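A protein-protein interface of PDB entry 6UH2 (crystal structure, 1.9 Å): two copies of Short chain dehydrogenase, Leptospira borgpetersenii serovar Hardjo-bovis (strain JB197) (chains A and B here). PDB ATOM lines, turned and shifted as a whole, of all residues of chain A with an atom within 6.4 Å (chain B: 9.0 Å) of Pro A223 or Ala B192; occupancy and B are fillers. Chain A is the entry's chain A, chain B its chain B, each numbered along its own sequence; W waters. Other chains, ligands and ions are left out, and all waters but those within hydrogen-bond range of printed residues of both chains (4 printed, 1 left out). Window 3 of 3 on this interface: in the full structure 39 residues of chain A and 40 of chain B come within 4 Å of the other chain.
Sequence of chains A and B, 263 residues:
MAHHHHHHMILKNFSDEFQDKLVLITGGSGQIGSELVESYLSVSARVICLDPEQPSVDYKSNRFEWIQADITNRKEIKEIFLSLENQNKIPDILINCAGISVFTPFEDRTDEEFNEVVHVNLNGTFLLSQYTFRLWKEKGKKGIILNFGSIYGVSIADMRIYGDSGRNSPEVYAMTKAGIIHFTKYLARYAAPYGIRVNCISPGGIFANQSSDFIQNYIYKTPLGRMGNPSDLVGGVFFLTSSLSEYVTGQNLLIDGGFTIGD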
ATOM      1  N   ILE A 219      18.440   7.917  31.560  1.00  0.00           N
ATOM      2  CA  ILE A 219      19.097   7.891  30.256  1.00  0.00           C
ATOM      3  C   ILE A 219      20.604   8.075  30.399  1.00  0.00           C
ATOM      4  O   ILE A 219      21.382   7.526  29.609  1.00  0.00           O
ATOM      5  CB  ILE A 219      18.464   8.959  29.341  1.00  0.00           C
ATOM      6  CG1 ILE A 219      17.073   8.500  28.891  1.00  0.00           C
ATOM      7  CG2 ILE A 219      19.358   9.272  28.148  1.00  0.00           C
ATOM      8  CD1 ILE A 219      16.309   9.538  28.091  1.00  0.00           C
ATOM      9  N   TYR A 220      21.043   8.827  31.416  1.00  0.00           N
ATOM     10  CA  TYR A 220      22.475   9.004  31.631  1.00  0.00           C
ATOM     11  C   TYR A 220      23.159   7.668  31.903  1.00  0.00           C
ATOM     12  O   TYR A 220      24.286   7.433  31.452  1.00  0.00           O
ATOM     13  CB  TYR A 220      22.717   9.980  32.783  1.00  0.00           C
ATOM     14  CG  TYR A 220      24.176  10.262  33.056  1.00  0.00           C
ATOM     15  CD1 TYR A 220      24.870  11.209  32.316  1.00  0.00           C
ATOM     16  CD2 TYR A 220      24.860   9.581  34.058  1.00  0.00           C
ATOM     17  CE1 TYR A 220      26.204  11.469  32.564  1.00  0.00           C
ATOM     18  CE2 TYR A 220      26.192   9.830  34.312  1.00  0.00           C
ATOM     19  CZ  TYR A 220      26.862  10.777  33.563  1.00  0.00           C
ATOM     20  OH  TYR A 220      28.191  11.033  33.813  1.00  0.00           O
ATOM     21  N   LYS A 221      22.489   6.776  32.629  1.00  0.00           N
ATOM     22  CA  LYS A 221      23.054   5.468  32.922  1.00  0.00           C
ATOM     23  C   LYS A 221      22.832   4.449  31.807  1.00  0.00           C
ATOM     24  O   LYS A 221      23.357   3.334  31.902  1.00  0.00           O
ATOM     25  CB  LYS A 221      22.466   4.937  34.231  1.00  0.00           C
ATOM     26  N   THR A 222      22.077   4.791  30.757  1.00  0.00           N
ATOM     27  CA  THR A 222      21.740   3.812  29.729  1.00  0.00           C
ATOM     28  C   THR A 222      22.610   4.033  28.499  1.00  0.00           C
ATOM     29  O   THR A 222      22.493   5.085  27.855  1.00  0.00           O
ATOM     30  CB  THR A 222      20.261   3.909  29.356  1.00  0.00           C
ATOM     31  OG1 THR A 222      19.468   3.876  30.546  1.00  0.00           O
ATOM     32  CG2 THR A 222      19.859   2.756  28.448  1.00  0.00           C
ATOM     33  N   PRO A 223      23.497   3.096  28.147  1.00  0.00           N
ATOM     34  CA  PRO A 223      24.350   3.304  26.957  1.00  0.00           C
ATOM     35  C   PRO A 223      23.581   3.653  25.686  1.00  0.00           C
ATOM     36  O   PRO A 223      23.967   4.590  24.977  1.00  0.00           O
ATOM     37  CB  PRO A 223      25.093   1.967  26.844  1.00  0.00           C
ATOM     38  CG  PRO A 223      25.207   1.491  28.280  1.00  0.00           C
ATOM     39  CD  PRO A 223      23.918   1.928  28.943  1.00  0.00           C
ATOM     40  N   LEU A 224      22.491   2.945  25.384  1.00  0.00           N
ATOM     41  CA  LEU A 224      21.741   3.253  24.172  1.00  0.00           C
ATOM     42  C   LEU A 224      20.990   4.579  24.260  1.00  0.00           C
ATOM     43  O   LEU A 224      20.341   4.969  23.282  1.00  0.00           O
ATOM     44  CB  LEU A 224      20.791   2.103  23.832  1.00  0.00           C
ATOM     45  CG  LEU A 224      21.551   0.819  23.471  1.00  0.00           C
ATOM     46  CD1 LEU A 224      20.649  -0.222  22.859  1.00  0.00           C
ATOM     47  CD2 LEU A 224      22.713   1.125  22.524  1.00  0.00           C
ATOM     48  N   GLY A 225      21.067   5.275  25.391  1.00  0.00           N
ATOM     49  CA  GLY A 225      20.683   6.672  25.440  1.00  0.00           C
ATOM     50  C   GLY A 225      19.199   6.952  25.372  1.00  0.00           C
ATOM     51  O   GLY A 225      18.807   8.038  24.947  1.00  0.00           O
ATOM     52  N   ARG A 226      18.361   6.009  25.792  1.00  0.00           N
ATOM     53  CA  ARG A 226      16.922   6.230  25.819  1.00  0.00           C
ATOM     54  C   ARG A 226      16.287   5.184  26.715  1.00  0.00           C
ATOM     55  O   ARG A 226      16.869   4.127  26.975  1.00  0.00           O
ATOM     56  CB  ARG A 226      16.299   6.154  24.418  1.00  0.00           C
ATOM     57  CG  ARG A 226      16.410   4.772  23.768  1.00  0.00           C
ATOM     58  CD  ARG A 226      15.521   4.698  22.526  1.00  0.00           C
ATOM     59  NE  ARG A 226      15.634   3.443  21.785  1.00  0.00           N
ATOM     60  CZ  ARG A 226      14.875   2.367  22.001  1.00  0.00           C
ATOM     61  NH1 ARG A 226      13.949   2.371  22.959  1.00  0.00           N
ATOM     62  NH2 ARG A 226      15.040   1.280  21.254  1.00  0.00           N
ATOM     63  N   ASP A 256      17.666  -3.852  28.045  1.00  0.00           N
ATOM     64  CA  ASP A 256      17.761  -2.645  28.863  1.00  0.00           C
ATOM     65  C   ASP A 256      18.677  -1.584  28.268  1.00  0.00           C
ATOM     66  O   ASP A 256      19.108  -0.685  29.002  1.00  0.00           O
ATOM     67  CB  ASP A 256      18.253  -2.991  30.295  1.00  0.00           C
ATOM     68  CG  ASP A 256      19.712  -3.468  30.342  1.00  0.00           C
ATOM     69  OD1 ASP A 256      20.329  -3.716  29.280  1.00  0.00           O
ATOM     70  OD2 ASP A 256      20.251  -3.594  31.472  1.00  0.00           O
ATOM     71  N   GLY A 257      18.999  -1.665  26.977  1.00  0.00           N
ATOM     72  CA  GLY A 257      19.893  -0.700  26.384  1.00  0.00           C
ATOM     73  C   GLY A 257      21.266  -0.654  27.014  1.00  0.00           C
ATOM     74  O   GLY A 257      21.969   0.336  26.849  1.00  0.00           O
ATOM     75  N   GLY A 258      21.676  -1.708  27.729  1.00  0.00           N
ATOM     76  CA  GLY A 258      22.975  -1.724  28.385  1.00  0.00           C
ATOM     77  C   GLY A 258      23.001  -1.164  29.796  1.00  0.00           C
ATOM     78  O   GLY A 258      24.096  -0.976  30.353  1.00  0.00           O
ATOM     79  N   PHE A 259      21.836  -0.900  30.392  1.00  0.00           N
ATOM     80  CA  PHE A 259      21.779  -0.325  31.739  1.00  0.00           C
ATOM     81  C   PHE A 259      22.639  -1.100  32.744  1.00  0.00           C
ATOM     82  O   PHE A 259      23.405  -0.504  33.508  1.00  0.00           O
ATOM     83  CB  PHE A 259      20.323  -0.276  32.215  1.00  0.00           C
ATOM     84  CG  PHE A 259      20.117   0.538  33.466  1.00  0.00           C
ATOM     85  CD1 PHE A 259      19.888   1.901  33.386  1.00  0.00           C
ATOM     86  CD2 PHE A 259      20.149  -0.059  34.716  1.00  0.00           C
ATOM     87  CE1 PHE A 259      19.698   2.662  34.524  1.00  0.00           C
ATOM     88  CE2 PHE A 259      19.958   0.700  35.867  1.00  0.00           C
ATOM     89  CZ  PHE A 259      19.733   2.062  35.765  1.00  0.00           C
ATOM     90  N   THR A 260      22.521  -2.428  32.768  1.00  0.00           N
ATOM     91  CA  THR A 260      23.133  -3.236  33.820  1.00  0.00           C
ATOM     92  C   THR A 260      24.516  -3.761  33.454  1.00  0.00           C
ATOM     93  O   THR A 260      24.948  -4.772  34.024  1.00  0.00           O
ATOM     94  CB  THR A 260      22.243  -4.431  34.176  1.00  0.00           C
ATOM     95  OG1 THR A 260      22.073  -5.259  33.016  1.00  0.00           O
ATOM     96  CG2 THR A 260      20.894  -3.975  34.692  1.00  0.00           C
ATOM     97  N   ILE A 261      25.216  -3.120  32.524  1.00  0.00           N
ATOM     98  CA  ILE A 261      26.502  -3.643  32.070  1.00  0.00           C
ATOM     99  C   ILE A 261      27.532  -3.610  33.194  1.00  0.00           C
ATOM    100  O   ILE A 261      27.478  -2.750  34.067  1.00  0.00           O
ATOM    101  CB  ILE A 261      27.010  -2.877  30.844  1.00  0.00           C
ATOM    102  CG1 ILE A 261      26.251  -3.308  29.594  1.00  0.00           C
ATOM    103  CG2 ILE A 261      28.485  -3.120  30.640  1.00  0.00           C
ATOM    104  CD1 ILE A 261      26.783  -2.661  28.336  1.00  0.00           C
ATOM    105  N   PHE B 133      35.097  -1.045  14.251  1.00  0.00           N
ATOM    106  CA  PHE B 133      34.660   0.143  14.985  1.00  0.00           C
ATOM    107  C   PHE B 133      35.154   1.429  14.328  1.00  0.00           C
ATOM    108  O   PHE B 133      34.378   2.367  14.117  1.00  0.00           O
ATOM    109  CB  PHE B 133      35.142   0.078  16.436  1.00  0.00           C
ATOM    110  CG  PHE B 133      34.829   1.317  17.229  1.00  0.00           C
ATOM    111  CD1 PHE B 133      33.549   1.537  17.718  1.00  0.00           C
ATOM    112  CD2 PHE B 133      35.811   2.270  17.470  1.00  0.00           C
ATOM    113  CE1 PHE B 133      33.258   2.681  18.447  1.00  0.00           C
ATOM    114  CE2 PHE B 133      35.526   3.409  18.206  1.00  0.00           C
ATOM    115  CZ  PHE B 133      34.247   3.612  18.694  1.00  0.00           C
ATOM    116  N   LYS B 142      25.638   2.290  11.707  1.00  0.00           N
ATOM    117  CA  LYS B 142      25.159   1.733  12.973  1.00  0.00           C
ATOM    118  C   LYS B 142      25.315   0.210  12.988  1.00  0.00           C
ATOM    119  O   LYS B 142      24.349  -0.545  13.053  1.00  0.00           O
ATOM    120  CB  LYS B 142      23.709   2.144  13.208  1.00  0.00           C
ATOM    121  N   GLY B 143      26.568  -0.233  12.940  1.00  0.00           N
ATOM    122  CA  GLY B 143      26.867  -1.651  12.818  1.00  0.00           C
ATOM    123  C   GLY B 143      26.537  -2.444  14.072  1.00  0.00           C
ATOM    124  O   GLY B 143      26.246  -1.895  15.137  1.00  0.00           O
ATOM    125  N   THR B 184      32.948  -7.879  25.360  1.00  0.00           N
ATOM    126  CA  THR B 184      31.634  -7.571  24.805  1.00  0.00           C
ATOM    127  C   THR B 184      30.946  -6.468  25.595  1.00  0.00           C
ATOM    128  O   THR B 184      30.395  -5.519  25.016  1.00  0.00           O
ATOM    129  CB  THR B 184      30.787  -8.836  24.804  1.00  0.00           C
ATOM    130  OG1 THR B 184      31.419  -9.827  23.987  1.00  0.00           O
ATOM    131  CG2 THR B 184      29.391  -8.547  24.290  1.00  0.00           C
ATOM    132  N   LYS B 185      30.951  -6.589  26.927  1.00  0.00           N
ATOM    133  CA  LYS B 185      30.377  -5.545  27.773  1.00  0.00           C
ATOM    134  C   LYS B 185      31.152  -4.245  27.638  1.00  0.00           C
ATOM    135  O   LYS B 185      30.558  -3.163  27.572  1.00  0.00           O
ATOM    136  CB  LYS B 185      30.366  -5.992  29.242  1.00  0.00           C
ATOM    137  CG  LYS B 185      29.627  -7.310  29.501  1.00  0.00           C
ATOM    138  CD  LYS B 185      29.706  -7.696  30.985  1.00  0.00           C
ATOM    139  CE  LYS B 185      28.696  -8.774  31.351  1.00  0.00           C
ATOM    140  NZ  LYS B 185      28.886  -9.989  30.539  1.00  0.00           N
ATOM    141  N   TYR B 186      32.482  -4.326  27.616  1.00  0.00           N
ATOM    142  CA  TYR B 186      33.289  -3.115  27.508  1.00  0.00           C
ATOM    143  C   TYR B 186      32.981  -2.357  26.223  1.00  0.00           C
ATOM    144  O   TYR B 186      32.741  -1.137  26.239  1.00  0.00           O
ATOM    145  CB  TYR B 186      34.768  -3.469  27.552  1.00  0.00           C
ATOM    146  CG  TYR B 186      35.676  -2.256  27.474  1.00  0.00           C
ATOM    147  CD1 TYR B 186      36.042  -1.707  26.235  1.00  0.00           C
ATOM    148  CD2 TYR B 186      36.167  -1.663  28.630  1.00  0.00           C
ATOM    149  CE1 TYR B 186      36.882  -0.601  26.159  1.00  0.00           C
ATOM    150  CE2 TYR B 186      37.018  -0.559  28.565  1.00  0.00           C
ATOM    151  CZ  TYR B 186      37.368  -0.033  27.329  1.00  0.00           C
ATOM    152  OH  TYR B 186      38.203   1.062  27.260  1.00  0.00           O
ATOM    153  N   LEU B 187      33.030  -3.060  25.090  1.00  0.00           N
ATOM    154  CA  LEU B 187      32.856  -2.384  23.815  1.00  0.00           C
ATOM    155  C   LEU B 187      31.411  -1.952  23.621  1.00  0.00           C
ATOM    156  O   LEU B 187      31.155  -0.913  22.996  1.00  0.00           O
ATOM    157  CB  LEU B 187      33.307  -3.291  22.674  1.00  0.00           C
ATOM    158  CG  LEU B 187      33.369  -2.559  21.329  1.00  0.00           C
ATOM    159  CD1 LEU B 187      34.370  -1.398  21.420  1.00  0.00           C
ATOM    160  CD2 LEU B 187      33.731  -3.525  20.232  1.00  0.00           C
ATOM    161  N   ALA B 188      30.456  -2.724  24.158  1.00  0.00           N
ATOM    162  CA  ALA B 188      29.062  -2.297  24.109  1.00  0.00           C
ATOM    163  C   ALA B 188      28.903  -0.919  24.731  1.00  0.00           C
ATOM    164  O   ALA B 188      28.223  -0.048  24.184  1.00  0.00           O
ATOM    165  CB  ALA B 188      28.173  -3.300  24.832  1.00  0.00           C
ATOM    166  N   ARG B 189      29.516  -0.709  25.893  1.00  0.00           N
ATOM    167  CA  ARG B 189      29.398   0.595  26.529  1.00  0.00           C
ATOM    168  C   ARG B 189      30.195   1.639  25.764  1.00  0.00           C
ATOM    169  O   ARG B 189      29.732   2.773  25.579  1.00  0.00           O
ATOM    170  CB  ARG B 189      29.861   0.517  27.986  1.00  0.00           C
ATOM    171  CG  ARG B 189      29.505   1.758  28.783  1.00  0.00           C
ATOM    172  CD  ARG B 189      29.774   1.576  30.264  1.00  0.00           C
ATOM    173  NE  ARG B 189      29.364   2.755  31.022  1.00  0.00           N
ATOM    174  CZ  ARG B 189      29.399   2.841  32.349  1.00  0.00           C
ATOM    175  NH1 ARG B 189      29.829   1.810  33.072  1.00  0.00           N
ATOM    176  NH2 ARG B 189      28.997   3.955  32.952  1.00  0.00           N
ATOM    177  N   TYR B 190      31.380   1.263  25.280  1.00  0.00           N
ATOM    178  CA  TYR B 190      32.250   2.208  24.580  1.00  0.00           C
ATOM    179  C   TYR B 190      31.654   2.649  23.247  1.00  0.00           C
ATOM    180  O   TYR B 190      31.724   3.835  22.888  1.00  0.00           O
ATOM    181  CB  TYR B 190      33.623   1.572  24.367  1.00  0.00           C
ATOM    182  CG  TYR B 190      34.715   2.549  23.960  1.00  0.00           C
ATOM    183  CD1 TYR B 190      35.445   3.243  24.917  1.00  0.00           C
ATOM    184  CD2 TYR B 190      35.009   2.778  22.612  1.00  0.00           C
ATOM    185  CE1 TYR B 190      36.449   4.131  24.555  1.00  0.00           C
ATOM    186  CE2 TYR B 190      36.019   3.663  22.242  1.00  0.00           C
ATOM    187  CZ  TYR B 190      36.729   4.333  23.216  1.00  0.00           C
ATOM    188  OH  TYR B 190      37.712   5.217  22.844  1.00  0.00           O
ATOM    189  N   ALA B 191      31.083   1.709  22.490  1.00  0.00           N
ATOM    190  CA  ALA B 191      30.601   1.984  21.143  1.00  0.00           C
ATOM    191  C   ALA B 191      29.159   2.471  21.101  1.00  0.00           C
ATOM    192  O   ALA B 191      28.713   2.930  20.043  1.00  0.00           O
ATOM    193  CB  ALA B 191      30.720   0.731  20.262  1.00  0.00           C
ATOM    194  N   ALA B 192      28.423   2.375  22.206  1.00  0.00           N
ATOM    195  CA  ALA B 192      27.022   2.789  22.212  1.00  0.00           C
ATOM    196  C   ALA B 192      26.781   4.220  21.741  1.00  0.00           C
ATOM    197  O   ALA B 192      25.792   4.430  21.019  1.00  0.00           O
ATOM    198  CB  ALA B 192      26.430   2.596  23.615  1.00  0.00           C
ATOM    199  N   PRO B 193      27.592   5.231  22.095  1.00  0.00           N
ATOM    200  CA  PRO B 193      27.312   6.599  21.606  1.00  0.00           C
ATOM    201  C   PRO B 193      27.296   6.715  20.096  1.00  0.00           C
ATOM    202  O   PRO B 193      26.712   7.671  19.567  1.00  0.00           O
ATOM    203  CB  PRO B 193      28.449   7.435  22.209  1.00  0.00           C
ATOM    204  CG  PRO B 193      28.910   6.670  23.391  1.00  0.00           C
ATOM    205  CD  PRO B 193      28.702   5.216  23.066  1.00  0.00           C
ATOM    206  N   TYR B 194      27.916   5.774  19.389  1.00  0.00           N
ATOM    207  CA  TYR B 194      27.929   5.723  17.936  1.00  0.00           C
ATOM    208  C   TYR B 194      26.848   4.817  17.361  1.00  0.00           C
ATOM    209  O   TYR B 194      26.889   4.505  16.168  1.00  0.00           O
ATOM    210  CB  TYR B 194      29.303   5.259  17.455  1.00  0.00           C
ATOM    211  CG  TYR B 194      30.410   6.100  18.043  1.00  0.00           C
ATOM    212  CD1 TYR B 194      30.773   7.307  17.456  1.00  0.00           C
ATOM    213  CD2 TYR B 194      31.070   5.704  19.204  1.00  0.00           C
ATOM    214  CE1 TYR B 194      31.778   8.093  17.997  1.00  0.00           C
ATOM    215  CE2 TYR B 194      32.078   6.481  19.749  1.00  0.00           C
ATOM    216  CZ  TYR B 194      32.426   7.671  19.136  1.00  0.00           C
ATOM    217  OH  TYR B 194      33.422   8.446  19.667  1.00  0.00           O
ATOM    218  N   GLY B 195      25.891   4.387  18.181  1.00  0.00           N
ATOM    219  CA  GLY B 195      24.806   3.554  17.701  1.00  0.00           C
ATOM    220  C   GLY B 195      25.191   2.135  17.347  1.00  0.00           C
ATOM    221  O   GLY B 195      24.457   1.469  16.613  1.00  0.00           O
ATOM    222  N   ILE B 196      26.333   1.661  17.835  1.00  0.00           N
ATOM    223  CA  ILE B 196      26.843   0.326  17.533  1.00  0.00           C
ATOM    224  C   ILE B 196      26.508  -0.579  18.709  1.00  0.00           C
ATOM    225  O   ILE B 196      26.827  -0.248  19.856  1.00  0.00           O
ATOM    226  CB  ILE B 196      28.363   0.370  17.274  1.00  0.00           C
ATOM    227  CG1 ILE B 196      28.660   1.118  15.971  1.00  0.00           C
ATOM    228  CG2 ILE B 196      28.989  -1.037  17.252  1.00  0.00           C
ATOM    229  CD1 ILE B 196      30.108   1.544  15.836  1.00  0.00           C
ATOM    230  N   ARG B 197      25.864  -1.716  18.436  1.00  0.00           N
ATOM    231  CA  ARG B 197      25.563  -2.707  19.463  1.00  0.00           C
ATOM    232  C   ARG B 197      26.589  -3.835  19.441  1.00  0.00           C
ATOM    233  O   ARG B 197      27.103  -4.208  18.383  1.00  0.00           O
ATOM    234  CB  ARG B 197      24.157  -3.300  19.273  1.00  0.00           C
ATOM    235  CG  ARG B 197      23.045  -2.265  19.339  1.00  0.00           C
ATOM    236  CD  ARG B 197      21.682  -2.909  19.550  1.00  0.00           C
ATOM    237  NE  ARG B 197      21.098  -3.472  18.323  1.00  0.00           N
ATOM    238  CZ  ARG B 197      20.879  -4.769  18.123  1.00  0.00           C
ATOM    239  NH1 ARG B 197      21.195  -5.658  19.072  1.00  0.00           N
ATOM    240  NH2 ARG B 197      20.314  -5.175  16.985  1.00  0.00           N
ATOM    241  N   VAL B 198      26.851  -4.408  20.621  1.00  0.00           N
ATOM    242  CA  VAL B 198      27.845  -5.468  20.787  1.00  0.00           C
ATOM    243  C   VAL B 198      27.274  -6.497  21.755  1.00  0.00           C
ATOM    244  O   VAL B 198      26.946  -6.154  22.899  1.00  0.00           O
ATOM    245  CB  VAL B 198      29.191  -4.948  21.322  1.00  0.00           C
ATOM    246  CG1 VAL B 198      30.238  -6.083  21.322  1.00  0.00           C
ATOM    247  CG2 VAL B 198      29.697  -3.709  20.524  1.00  0.00           C
ATOM    248  N   GLU B 246      16.919  -4.452  18.987  1.00  0.00           N
ATOM    249  CA  GLU B 246      17.388  -3.059  18.931  1.00  0.00           C
ATOM    250  C   GLU B 246      17.817  -2.492  20.283  1.00  0.00           C
ATOM    251  O   GLU B 246      18.687  -1.611  20.340  1.00  0.00           O
ATOM    252  CB  GLU B 246      16.287  -2.147  18.373  1.00  0.00           C
ATOM    253  CG  GLU B 246      16.177  -2.139  16.878  1.00  0.00           C
ATOM    254  CD  GLU B 246      15.111  -1.171  16.372  1.00  0.00           C
ATOM    255  OE1 GLU B 246      15.040  -0.971  15.140  1.00  0.00           O
ATOM    256  OE2 GLU B 246      14.343  -0.620  17.199  1.00  0.00           O
ATOM    257  N   TYR B 247      17.186  -2.928  21.370  1.00  0.00           N
ATOM    258  CA  TYR B 247      17.464  -2.383  22.693  1.00  0.00           C
ATOM    259  C   TYR B 247      18.319  -3.334  23.538  1.00  0.00           C
ATOM    260  O   TYR B 247      18.357  -3.207  24.765  1.00  0.00           O
ATOM    261  CB  TYR B 247      16.142  -2.049  23.398  1.00  0.00           C
ATOM    262  CG  TYR B 247      16.200  -1.054  24.551  1.00  0.00           C
ATOM    263  CD1 TYR B 247      16.724   0.225  24.378  1.00  0.00           C
ATOM    264  CD2 TYR B 247      15.672  -1.379  25.805  1.00  0.00           C
ATOM    265  CE1 TYR B 247      16.748   1.143  25.438  1.00  0.00           C
ATOM    266  CE2 TYR B 247      15.688  -0.464  26.869  1.00  0.00           C
ATOM    267  CZ  TYR B 247      16.220   0.790  26.682  1.00  0.00           C
ATOM    268  OH  TYR B 247      16.241   1.688  27.740  1.00  0.00           O
ATOM    269  N   VAL B 248      19.020  -4.271  22.901  1.00  0.00           N
ATOM    270  CA  VAL B 248      19.847  -5.256  23.594  1.00  0.00           C
ATOM    271  C   VAL B 248      21.302  -4.996  23.235  1.00  0.00           C
ATOM    272  O   VAL B 248      21.688  -5.123  22.067  1.00  0.00           O
ATOM    273  CB  VAL B 248      19.455  -6.694  23.214  1.00  0.00           C
ATOM    274  CG1 VAL B 248      20.310  -7.701  23.997  1.00  0.00           C
ATOM    275  CG2 VAL B 248      17.976  -6.947  23.452  1.00  0.00           C
ATOM    276  N   THR B 249      22.122  -4.663  24.229  1.00  0.00           N
ATOM    277  CA  THR B 249      23.548  -4.524  23.970  1.00  0.00           C
ATOM    278  C   THR B 249      24.324  -4.907  25.229  1.00  0.00           C
ATOM    279  O   THR B 249      23.837  -4.751  26.351  1.00  0.00           O
ATOM    280  CB  THR B 249      23.912  -3.105  23.487  1.00  0.00           C
ATOM    281  OG1 THR B 249      25.241  -3.103  22.945  1.00  0.00           O
ATOM    282  CG2 THR B 249      23.837  -2.074  24.625  1.00  0.00           C
ATOM    283  N   GLY B 250      25.525  -5.444  25.027  1.00  0.00           N
ATOM    284  CA  GLY B 250      26.362  -5.856  26.143  1.00  0.00           C
ATOM    285  C   GLY B 250      26.033  -7.202  26.749  1.00  0.00           C
ATOM    286  O   GLY B 250      26.593  -7.540  27.797  1.00  0.00           O
ATOM    287  N   GLN B 251      25.183  -7.999  26.113  1.00  0.00           N
ATOM    288  CA  GLN B 251      24.679  -9.221  26.720  1.00  0.00           C
ATOM    289  C   GLN B 251      25.434 -10.444  26.212  1.00  0.00           C
ATOM    290  O   GLN B 251      25.908 -10.472  25.076  1.00  0.00           O
ATOM    291  CB  GLN B 251      23.181  -9.371  26.443  1.00  0.00           C
ATOM    292  CG  GLN B 251      22.371  -8.143  26.900  1.00  0.00           C
ATOM    293  CD  GLN B 251      22.657  -7.746  28.338  1.00  0.00           C
ATOM    294  OE1 GLN B 251      22.516  -8.553  29.249  1.00  0.00           O
ATOM    295  NE2 GLN B 251      23.074  -6.493  28.547  1.00  0.00           N
HETATM  296  O   HOH W   1      20.307  -5.247  27.049  1.00  0.00           O
HETATM  297  O   HOH W   2      22.906  -4.501  30.321  1.00  0.00           O
HETATM  298  O   HOH W   3      16.900   0.515  30.254  1.00  0.00           O
HETATM  299  O   HOH W   4      22.900   5.225  21.167  1.00  0.00           O
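Of chain B, only Ala B192 (3.4 Å) comes within 4 Å of Pro A223.
Of the printed residues of chain B, Arg A226 touches Tyr B247.
Of chain B, only Thr B249 comes within 4 Å of Gly A258.
Printed residues of chain B within 4 Å of Ile A261: Lys B185 (3.7 Å), Ala B188 (3.8 Å) and Gly B250 (3.9 Å).
Printed residues of chain A within 4 Å of Glu B246: Leu A224.
Printed residues of chain A within 4 Å of Tyr B247: Thr A222, Leu A224, Arg A226, Asp A256 and Gly A257.
Of the printed residues of chain A, Gln B251 touches Asp A256.
The nearest residue of chain B that does not touch Pro A223 is Arg B189 (4.3 Å).
The nearest printed residue of chain B that does not touch Ile A261 is Thr B249 (4.1 Å).
Water W2 lies within hydrogen-bond range of NE2 of Gln B251 (2.7 Å), OD1 of Asp A256 (2.9 Å), OG1 of Thr A260 (2.9 Å) and N of Ile A261 (3.5 Å).
Water W1 lies within hydrogen-bond range of the side-chain carboxylate (OD1) of Asp A256, the side-chain amide nitrogen (NE2) of Gln B251 and the backbone NH (N) of Thr B249.
Water W3 lies within hydrogen-bond range of the backbone carbonyl oxygen of Asp A256 (2.8 Å) and the side-chain hydroxyl of Tyr B247 (2.9 Å).
Water W4 bridges the backbone carbonyl oxygen (O) of Ala B192 and the backbone carbonyl oxygen (O) of Leu A224.
Hydrophobic or aromatic side chains of chain B within 4 Å of the printed part of chain A: Ala B188, Ala B192 and Tyr B247.
Among the printed residues, no Asp or Glu carboxylate lies within 4 Å of a Lys or Arg side-chain nitrogen of the other chain.
The backbone carbonyl oxygen (O) of Gly A257 is in hydrogen-bond range of the backbone NH (N) of Leu A224 (3.0 Å).
The side-chain carboxylate (OD1) of Asp A256 lies within hydrogen-bond range of the backbone NH (N) of Gly A258, 2.9 Å away.
N of Phe A259 sits at hydrogen-bond distance from OD2 of Asp A256, 3.3 Å away.
OD2 of Asp A256 sits at hydrogen-bond distance from N of Thr A260, 2.9 Å away.
The backbone NH (N) of Val B198 sits at hydrogen-bond distance from the side-chain hydroxyl (OG1) of Thr B249.
O of Val B198 lies within hydrogen-bond range of N of Gly B250, 2.7 Å away.
OH of Tyr B247 lies within hydrogen-bond range of O of Arg A226 (2.6 Å).
N of Asp A256 sits at hydrogen-bond distance from O of Tyr B247, at 3.4 Å.
The backbone carbonyl oxygen (O) of Tyr B247 lies within hydrogen-bond range of the backbone NH (N) of Gly A257.
No position is printed for both chains.
Thr A222 touches Tyr B247.
O of Pro A223 touches CB of Ala B192 (3.4 Å).
Glu B246 touches Leu A224.
CD1 of Leu A224 touches CA of Tyr B247 (3.9 Å).
Asp A256 touches Gln B251 (OD1 to NE2, 3.97 Å).
CG2 of Thr B249 touches O of Gly A257 (3.8 Å).
Gly A258 touches Thr B249.
CG2 of Ile A261 touches O of Lys B185, 3.7 Å away.
CD1 of Ile A261 touches CB of Ala B188, at 3.8 Å.
Gly B250 touches Ile A261 (CA to CD1, 3.9 Å).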
